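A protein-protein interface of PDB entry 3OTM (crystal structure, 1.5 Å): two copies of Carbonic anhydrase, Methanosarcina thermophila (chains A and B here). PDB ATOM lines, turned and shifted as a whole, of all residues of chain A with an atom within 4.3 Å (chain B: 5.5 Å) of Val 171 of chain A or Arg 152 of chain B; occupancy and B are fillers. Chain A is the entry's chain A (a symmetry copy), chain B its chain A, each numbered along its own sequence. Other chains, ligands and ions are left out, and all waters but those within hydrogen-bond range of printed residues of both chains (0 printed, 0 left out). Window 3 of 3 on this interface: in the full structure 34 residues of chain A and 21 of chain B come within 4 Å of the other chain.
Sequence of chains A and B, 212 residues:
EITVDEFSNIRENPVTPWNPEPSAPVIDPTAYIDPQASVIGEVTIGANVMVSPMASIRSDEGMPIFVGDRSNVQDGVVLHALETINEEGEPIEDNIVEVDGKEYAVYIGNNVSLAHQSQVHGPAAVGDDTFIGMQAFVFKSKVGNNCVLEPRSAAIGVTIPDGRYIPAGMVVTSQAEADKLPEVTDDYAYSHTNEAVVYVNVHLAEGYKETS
Ala 136 of chain A touches Arg 152 of chain B, but with the chains exchanged Arg 152 of chain A does not touch Ala 136 of chain B (10.2 Å).
Arg 152 of chain B touches its own counterpart, Arg 152 of chain A.
Ala 154 of chain A touches Arg 152 of chain B, but with the chains exchanged Arg 152 of chain A does not touch Ala 154 of chain B (9.8 Å).
Val 171 of chain A touches Arg 152 of chain B, but with the chains exchanged Arg 152 of chain A does not touch Val 171 of chain B (7.8 Å).
Of the 12 pairs that touch across the chains among the printed residues, 2 have their exchanged pair printed and touching as well.
The side-chain amide nitrogen of Gln 135 of chain B lies within hydrogen-bond range of the backbone carbonyl oxygen of Ala 136 of chain A (3.3 Å).
NH2 of Arg 152 of chain B sits at hydrogen-bond distance from O of Gln 135 of chain A, at 2.7 Å.
NH1 of Arg 152 of chain B lies within hydrogen-bond range of O of Arg 152 of chain A (2.9 Å).
The backbone carbonyl oxygen of Ser 153 of chain A is in hydrogen-bond range of the guanidinium group of Arg 152 of chain B, at 3.1 Å.
O of Gln 135 of chain A touches OE1 of Gln 135 of chain B, 3.7 Å away.
Ala 136 of chain A touches Arg 152 of chain B (CA to NH2, 3.6 Å).
CB of Met 134 of chain B touches CE1 of Phe 137 of chain A, 3.6 Å away.
Gln 135 of chain B touches Phe 137 of chain A (OE1 to CB, 3.4 Å).
Pro 151 of chain B touches Phe 137 of chain A (CB to CE2, 3.5 Å).
NH2 of Arg 152 of chain B touches N of Phe 137 of chain A, at 3.7 Å.
Ala 154 of chain A touches Arg 152 of chain B (CB to NH1, 3.99 Å).
CG2 of Val 171 of chain A touches NH1 of Arg 152 of chain B, at 3.96 Å.
Of the 13 printed residues of chain B, 4 touch a printed residue of chain A.
Hydrophobic or aromatic side chains of chain B that line the printed part of chain A: Met 134 and Pro 151.
Of the 12 printed residues of chain A, 7 touch a printed residue of chain B.
Printed residues of chain A that touch a printed residue of chain B: Gln 135, Ala 136, Phe 137, Arg 152, Ser 153, Ala 154 and Val 171.
Hydrophobic or aromatic side chains of chain A that line the printed part of chain B: Phe 137, Ala 154 and Val 171.
Among the printed residues, 12 pairs touch across the chains.
Among the printed residues, no Asp or Glu carboxylate lies within 4 Å of a Lys or Arg side-chain nitrogen of the other chain.
O of Met 134 of chain B lies within hydrogen-bond range of N of Arg 152 of chain B (2.9 Å).
NE of Arg 152 of chain B is in hydrogen-bond range of OE1 of Gln 135 of chain B, at 2.7 Å.
The backbone carbonyl oxygen of Pro 151 of chain B lies within hydrogen-bond range of the backbone NH of Gly 169 of chain B.
The backbone carbonyl oxygen (O) of Ser 153 of chain A lies within hydrogen-bond range of the backbone NH (N) of Phe 137 of chain A (3.1 Å).
N of Ala 154 of chain A lies within hydrogen-bond range of O of Met 170 of chain A (2.9 Å).
O of Ala 154 of chain A sits at hydrogen-bond distance from N of Val 172 of chain A, 2.9 Å away.
Val 171 of chain A touches just one residue of chain B: Arg 152 (3.96 Å).
Of the printed residues of chain A, Met 134 of chain B touches Phe 137 (3.6 Å).
Printed residues of chain A within 4 Å of Pro 151 of chain B: Phe 137 (3.5 Å).
Val 171 of chain B touches none of the printed residues of chain A.
The nearest residue of chain B that does not touch Val 171 of chain A is Gly 169 of chain B (4.3 Å).
The nearest printed residue of chain A that does not touch Arg 152 of chain B is Gly 169 of chain A (5.1 Å).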
ATOM      1  N   GLN A 135      10.865 -12.486  20.627  1.00  0.00           N
ATOM      2  CA  GLN A 135      10.557 -12.012  21.986  1.00  0.00           C
ATOM      3  C   GLN A 135       9.093 -11.609  22.189  1.00  0.00           C
ATOM      4  O   GLN A 135       8.787 -10.960  23.165  1.00  0.00           O
ATOM      5  CB  GLN A 135      11.485 -10.869  22.417  1.00  0.00           C
ATOM      6  CG  GLN A 135      12.955 -11.293  22.529  1.00  0.00           C
ATOM      7  CD  GLN A 135      13.870 -10.207  23.018  1.00  0.00           C
ATOM      8  OE1 GLN A 135      13.497  -9.045  23.072  1.00  0.00           O
ATOM      9  NE2 GLN A 135      15.095 -10.569  23.349  1.00  0.00           N
ATOM     10  N   ALA A 136       8.207 -11.951  21.279  1.00  0.00           N
ATOM     11  CA  ALA A 136       6.796 -11.578  21.414  1.00  0.00           C
ATOM     12  C   ALA A 136       6.089 -12.515  22.387  1.00  0.00           C
ATOM     13  O   ALA A 136       6.633 -13.557  22.792  1.00  0.00           O
ATOM     14  CB  ALA A 136       6.116 -11.574  20.055  1.00  0.00           C
ATOM     15  N   PHE A 137       4.865 -12.152  22.777  1.00  0.00           N
ATOM     16  CA  PHE A 137       4.147 -12.875  23.811  1.00  0.00           C
ATOM     17  C   PHE A 137       2.676 -12.899  23.447  1.00  0.00           C
ATOM     18  O   PHE A 137       2.106 -11.858  23.129  1.00  0.00           O
ATOM     19  CB  PHE A 137       4.343 -12.196  25.170  1.00  0.00           C
ATOM     20  CG  PHE A 137       3.648 -12.867  26.298  1.00  0.00           C
ATOM     21  CD1 PHE A 137       4.008 -14.136  26.709  1.00  0.00           C
ATOM     22  CD2 PHE A 137       2.651 -12.201  26.987  1.00  0.00           C
ATOM     23  CE1 PHE A 137       3.358 -14.746  27.767  1.00  0.00           C
ATOM     24  CE2 PHE A 137       2.000 -12.808  28.026  1.00  0.00           C
ATOM     25  CZ  PHE A 137       2.351 -14.073  28.428  1.00  0.00           C
ATOM     26  N   ARG A 152       8.961  -8.064  20.077  1.00  0.00           N
ATOM     27  CA  ARG A 152       8.635  -7.442  21.357  1.00  0.00           C
ATOM     28  C   ARG A 152       7.203  -6.981  21.521  1.00  0.00           C
ATOM     29  O   ARG A 152       6.912  -6.325  22.501  1.00  0.00           O
ATOM     30  CB  ARG A 152       9.552  -6.248  21.597  1.00  0.00           C
ATOM     31  CG  ARG A 152      10.819  -6.633  22.162  1.00  0.00           C
ATOM     32  CD  ARG A 152      10.674  -6.878  23.615  1.00  0.00           C
ATOM     33  NE  ARG A 152      12.042  -6.935  24.015  1.00  0.00           N
ATOM     34  CZ  ARG A 152      12.772  -5.879  24.301  1.00  0.00           C
ATOM     35  NH1 ARG A 152      12.242  -4.648  24.365  1.00  0.00           N
ATOM     36  NH2 ARG A 152      14.031  -6.089  24.568  1.00  0.00           N
ATOM     37  N   SER A 153       6.321  -7.303  20.580  1.00  0.00           N
ATOM     38  CA  SER A 153       4.889  -7.016  20.762  1.00  0.00           C
ATOM     39  C   SER A 153       4.231  -8.093  21.646  1.00  0.00           C
ATOM     40  O   SER A 153       4.812  -9.154  21.913  1.00  0.00           O
ATOM     41  CB  SER A 153       4.183  -6.903  19.415  1.00  0.00           C
ATOM     42  OG  SER A 153       4.149  -8.145  18.733  1.00  0.00           O
ATOM     43  N   ALA A 154       3.030  -7.817  22.121  1.00  0.00           N
ATOM     44  CA  ALA A 154       2.303  -8.762  22.942  1.00  0.00           C
ATOM     45  C   ALA A 154       0.806  -8.585  22.767  1.00  0.00           C
ATOM     46  O   ALA A 154       0.327  -7.471  22.550  1.00  0.00           O
ATOM     47  CB  ALA A 154       2.678  -8.612  24.397  1.00  0.00           C
ATOM     48  N   GLY A 169       7.086  -3.647  20.130  1.00  0.00           N
ATOM     49  CA  GLY A 169       7.076  -3.132  21.482  1.00  0.00           C
ATOM     50  C   GLY A 169       5.701  -2.873  22.064  1.00  0.00           C
ATOM     51  O   GLY A 169       5.590  -2.643  23.261  1.00  0.00           O
ATOM     52  N   MET A 170       4.668  -2.878  21.219  1.00  0.00           N
ATOM     53  CA  MET A 170       3.304  -2.599  21.673  1.00  0.00           C
ATOM     54  C   MET A 170       2.705  -3.785  22.433  1.00  0.00           C
ATOM     55  O   MET A 170       2.787  -4.931  21.997  1.00  0.00           O
ATOM     56  CB  MET A 170       2.410  -2.212  20.493  1.00  0.00           C
ATOM     57  CG  MET A 170       0.984  -1.830  20.882  1.00  0.00           C
ATOM     58  SD  MET A 170      -0.020  -1.372  19.452  1.00  0.00           S
ATOM     59  CE  MET A 170       1.050  -0.131  18.738  1.00  0.00           C
ATOM     60  N   VAL A 171       2.117  -3.487  23.584  1.00  0.00           N
ATOM     61  CA  VAL A 171       1.444  -4.479  24.399  1.00  0.00           C
ATOM     62  C   VAL A 171      -0.050  -4.182  24.353  1.00  0.00           C
ATOM     63  O   VAL A 171      -0.504  -3.135  24.834  1.00  0.00           O
ATOM     64  CB  VAL A 171       1.957  -4.434  25.842  1.00  0.00           C
ATOM     65  CG1 VAL A 171       1.187  -5.406  26.706  1.00  0.00           C
ATOM     66  CG2 VAL A 171       3.451  -4.756  25.884  1.00  0.00           C
ATOM     67  N   VAL A 172      -0.799  -5.072  23.719  1.00  0.00           N
ATOM     68  CA  VAL A 172      -2.226  -4.889  23.465  1.00  0.00           C
ATOM     69  C   VAL A 172      -3.001  -5.719  24.480  1.00  0.00           C
ATOM     70  O   VAL A 172      -2.880  -6.949  24.517  1.00  0.00           O
ATOM     71  CB  VAL A 172      -2.584  -5.321  22.056  1.00  0.00           C
ATOM     72  CG1 VAL A 172      -4.095  -5.187  21.788  1.00  0.00           C
ATOM     73  CG2 VAL A 172      -1.757  -4.529  21.013  1.00  0.00           C
ATOM     74  N   THR A 173      -3.770  -5.047  25.324  1.00  0.00           N
ATOM     75  CA  THR A 173      -4.502  -5.720  26.398  1.00  0.00           C
ATOM     76  C   THR A 173      -5.998  -5.416  26.362  1.00  0.00           C
ATOM     77  O   THR A 173      -6.751  -5.923  27.187  1.00  0.00           O
ATOM     78  CB  THR A 173      -3.995  -5.275  27.785  1.00  0.00           C
ATOM     79  OG1 THR A 173      -4.136  -3.860  27.891  1.00  0.00           O
ATOM     80  CG2 THR A 173      -2.524  -5.690  28.008  1.00  0.00           C
ATOM     81  N   GLU A 177      -8.301  -1.608  21.503  1.00  0.00           N
ATOM     82  CA  GLU A 177      -7.004  -1.431  20.850  1.00  0.00           C
ATOM     83  C   GLU A 177      -6.852  -2.412  19.695  1.00  0.00           C
ATOM     84  O   GLU A 177      -6.404  -2.053  18.616  1.00  0.00           O
ATOM     85  CB  GLU A 177      -5.845  -1.761  21.798  1.00  0.00           C
ATOM     86  CG  GLU A 177      -5.600  -0.867  22.994  1.00  0.00           C
ATOM     87  CD  GLU A 177      -4.324  -1.292  23.745  1.00  0.00           C
ATOM     88  OE1 GLU A 177      -3.245  -0.735  23.439  1.00  0.00           O
ATOM     89  OE2 GLU A 177      -4.390  -2.202  24.608  1.00  0.00           O
ATOM     90  N   GLY B 133       5.552 -12.690  36.577  1.00  0.00           N
ATOM     91  CA  GLY B 133       4.914 -13.157  35.366  1.00  0.00           C
ATOM     92  C   GLY B 133       5.837 -13.439  34.213  1.00  0.00           C
ATOM     93  O   GLY B 133       7.042 -13.176  34.223  1.00  0.00           O
ATOM     94  N   MET B 134       5.226 -13.979  33.168  1.00  0.00           N
ATOM     95  CA  MET B 134       5.962 -14.426  31.993  1.00  0.00           C
ATOM     96  C   MET B 134       6.757 -13.285  31.399  1.00  0.00           C
ATOM     97  O   MET B 134       6.255 -12.181  31.230  1.00  0.00           O
ATOM     98  CB  MET B 134       4.996 -14.968  30.933  1.00  0.00           C
ATOM     99  CG  MET B 134       4.229 -16.230  31.318  1.00  0.00           C
ATOM    100  SD  MET B 134       2.701 -15.745  32.198  1.00  0.00           S
ATOM    101  CE  MET B 134       1.838 -17.298  32.415  1.00  0.00           C
ATOM    102  N   GLN B 135       8.021 -13.552  31.101  1.00  0.00           N
ATOM    103  CA  GLN B 135       8.923 -12.570  30.477  1.00  0.00           C
ATOM    104  C   GLN B 135       9.217 -11.349  31.355  1.00  0.00           C
ATOM    105  O   GLN B 135       9.715 -10.365  30.853  1.00  0.00           O
ATOM    106  CB  GLN B 135       8.416 -12.122  29.101  1.00  0.00           C
ATOM    107  CG  GLN B 135       8.384 -13.258  28.069  1.00  0.00           C
ATOM    108  CD  GLN B 135       7.959 -12.826  26.695  1.00  0.00           C
ATOM    109  OE1 GLN B 135       7.454 -11.729  26.507  1.00  0.00           O
ATOM    110  NE2 GLN B 135       8.126 -13.699  25.721  1.00  0.00           N
ATOM    111  N   ALA B 136       8.890 -11.387  32.628  1.00  0.00           N
ATOM    112  CA  ALA B 136       9.134 -10.242  33.510  1.00  0.00           C
ATOM    113  C   ALA B 136      10.597 -10.199  33.935  1.00  0.00           C
ATOM    114  O   ALA B 136      11.363 -11.154  33.714  1.00  0.00           O
ATOM    115  CB  ALA B 136       8.209 -10.292  34.714  1.00  0.00           C
ATOM    116  N   GLU B 150       2.836  -8.538  36.371  1.00  0.00           N
ATOM    117  CA  GLU B 150       2.153  -9.089  35.212  1.00  0.00           C
ATOM    118  C   GLU B 150       3.165  -9.384  34.129  1.00  0.00           C
ATOM    119  O   GLU B 150       4.303  -8.913  34.172  1.00  0.00           O
ATOM    120  CB  GLU B 150       1.079  -8.115  34.706  1.00  0.00           C
ATOM    121  CG  GLU B 150      -0.106  -8.018  35.657  1.00  0.00           C
ATOM    122  CD  GLU B 150      -1.258  -7.215  35.108  1.00  0.00           C
ATOM    123  OE1 GLU B 150      -1.255  -6.920  33.907  1.00  0.00           O
ATOM    124  OE2 GLU B 150      -2.178  -6.877  35.911  1.00  0.00           O
ATOM    125  N   PRO B 151       2.751 -10.158  33.131  1.00  0.00           N
ATOM    126  CA  PRO B 151       3.696 -10.469  32.044  1.00  0.00           C
ATOM    127  C   PRO B 151       4.334  -9.236  31.464  1.00  0.00           C
ATOM    128  O   PRO B 151       3.672  -8.204  31.292  1.00  0.00           O
ATOM    129  CB  PRO B 151       2.811 -11.177  31.011  1.00  0.00           C
ATOM    130  CG  PRO B 151       1.765 -11.822  31.818  1.00  0.00           C
ATOM    131  CD  PRO B 151       1.462 -10.821  32.939  1.00  0.00           C
ATOM    132  N   ARG B 152       5.612  -9.348  31.138  1.00  0.00           N
ATOM    133  CA  ARG B 152       6.374  -8.272  30.510  1.00  0.00           C
ATOM    134  C   ARG B 152       6.597  -7.039  31.360  1.00  0.00           C
ATOM    135  O   ARG B 152       7.091  -6.057  30.842  1.00  0.00           O
ATOM    136  CB  ARG B 152       5.689  -7.843  29.218  1.00  0.00           C
ATOM    137  CG  ARG B 152       6.047  -8.680  28.103  1.00  0.00           C
ATOM    138  CD  ARG B 152       7.379  -8.295  27.584  1.00  0.00           C
ATOM    139  NE  ARG B 152       7.400  -9.003  26.347  1.00  0.00           N
ATOM    140  CZ  ARG B 152       6.873  -8.553  25.229  1.00  0.00           C
ATOM    141  NH1 ARG B 152       6.376  -7.310  25.131  1.00  0.00           N
ATOM    142  NH2 ARG B 152       6.898  -9.355  24.201  1.00  0.00           N
ATOM    143  N   SER B 153       6.234  -7.075  32.639  1.00  0.00           N
ATOM    144  CA  SER B 153       6.567  -5.965  33.546  1.00  0.00           C
ATOM    145  C   SER B 153       8.025  -6.085  34.032  1.00  0.00           C
ATOM    146  O   SER B 153       8.681  -7.122  33.859  1.00  0.00           O
ATOM    147  CB  SER B 153       5.597  -5.917  34.722  1.00  0.00           C
ATOM    148  OG  SER B 153       5.742  -7.043  35.570  1.00  0.00           O
ATOM    149  N   ALA B 154       8.542  -5.021  34.619  1.00  0.00           N
ATOM    150  CA  ALA B 154       9.894  -5.024  35.138  1.00  0.00           C
ATOM    151  C   ALA B 154      10.018  -4.077  36.317  1.00  0.00           C
ATOM    152  O   ALA B 154       9.348  -3.044  36.365  1.00  0.00           O
ATOM    153  CB  ALA B 154      10.885  -4.648  34.062  1.00  0.00           C
ATOM    154  N   ALA B 168       0.923  -5.195  33.033  1.00  0.00           N
ATOM    155  CA  ALA B 168       1.667  -5.764  31.920  1.00  0.00           C
ATOM    156  C   ALA B 168       2.404  -4.707  31.117  1.00  0.00           C
ATOM    157  O   ALA B 168       1.819  -3.684  30.736  1.00  0.00           O
ATOM    158  CB  ALA B 168       0.725  -6.536  31.001  1.00  0.00           C
ATOM    159  N   GLY B 169       3.681  -4.964  30.855  1.00  0.00           N
ATOM    160  CA  GLY B 169       4.483  -4.127  29.988  1.00  0.00           C
ATOM    161  C   GLY B 169       5.138  -2.939  30.662  1.00  0.00           C
ATOM    162  O   GLY B 169       5.995  -2.307  30.061  1.00  0.00           O
ATOM    163  N   MET B 170       4.713  -2.620  31.887  1.00  0.00           N
ATOM    164  CA  MET B 170       5.253  -1.466  32.609  1.00  0.00           C
ATOM    165  C   MET B 170       6.656  -1.742  33.153  1.00  0.00           C
ATOM    166  O   MET B 170       6.917  -2.783  33.750  1.00  0.00           O
ATOM    167  CB  MET B 170       4.312  -1.049  33.741  1.00  0.00           C
ATOM    168  CG  MET B 170       4.757   0.196  34.503  1.00  0.00           C
ATOM    169  SD  MET B 170       3.603   0.646  35.819  1.00  0.00           S
ATOM    170  CE  MET B 170       2.093   0.704  34.866  1.00  0.00           C
ATOM    171  N   VAL B 171       7.555  -0.796  32.918  1.00  0.00           N
ATOM    172  CA  VAL B 171       8.914  -0.866  33.417  1.00  0.00           C
ATOM    173  C   VAL B 171       9.075   0.211  34.483  1.00  0.00           C
ATOM    174  O   VAL B 171       8.994   1.411  34.189  1.00  0.00           O
ATOM    175  CB  VAL B 171       9.920  -0.653  32.282  1.00  0.00           C
ATOM    176  CG1 VAL B 171      11.332  -0.636  32.823  1.00  0.00           C
ATOM    177  CG2 VAL B 171       9.771  -1.750  31.228  1.00  0.00           C
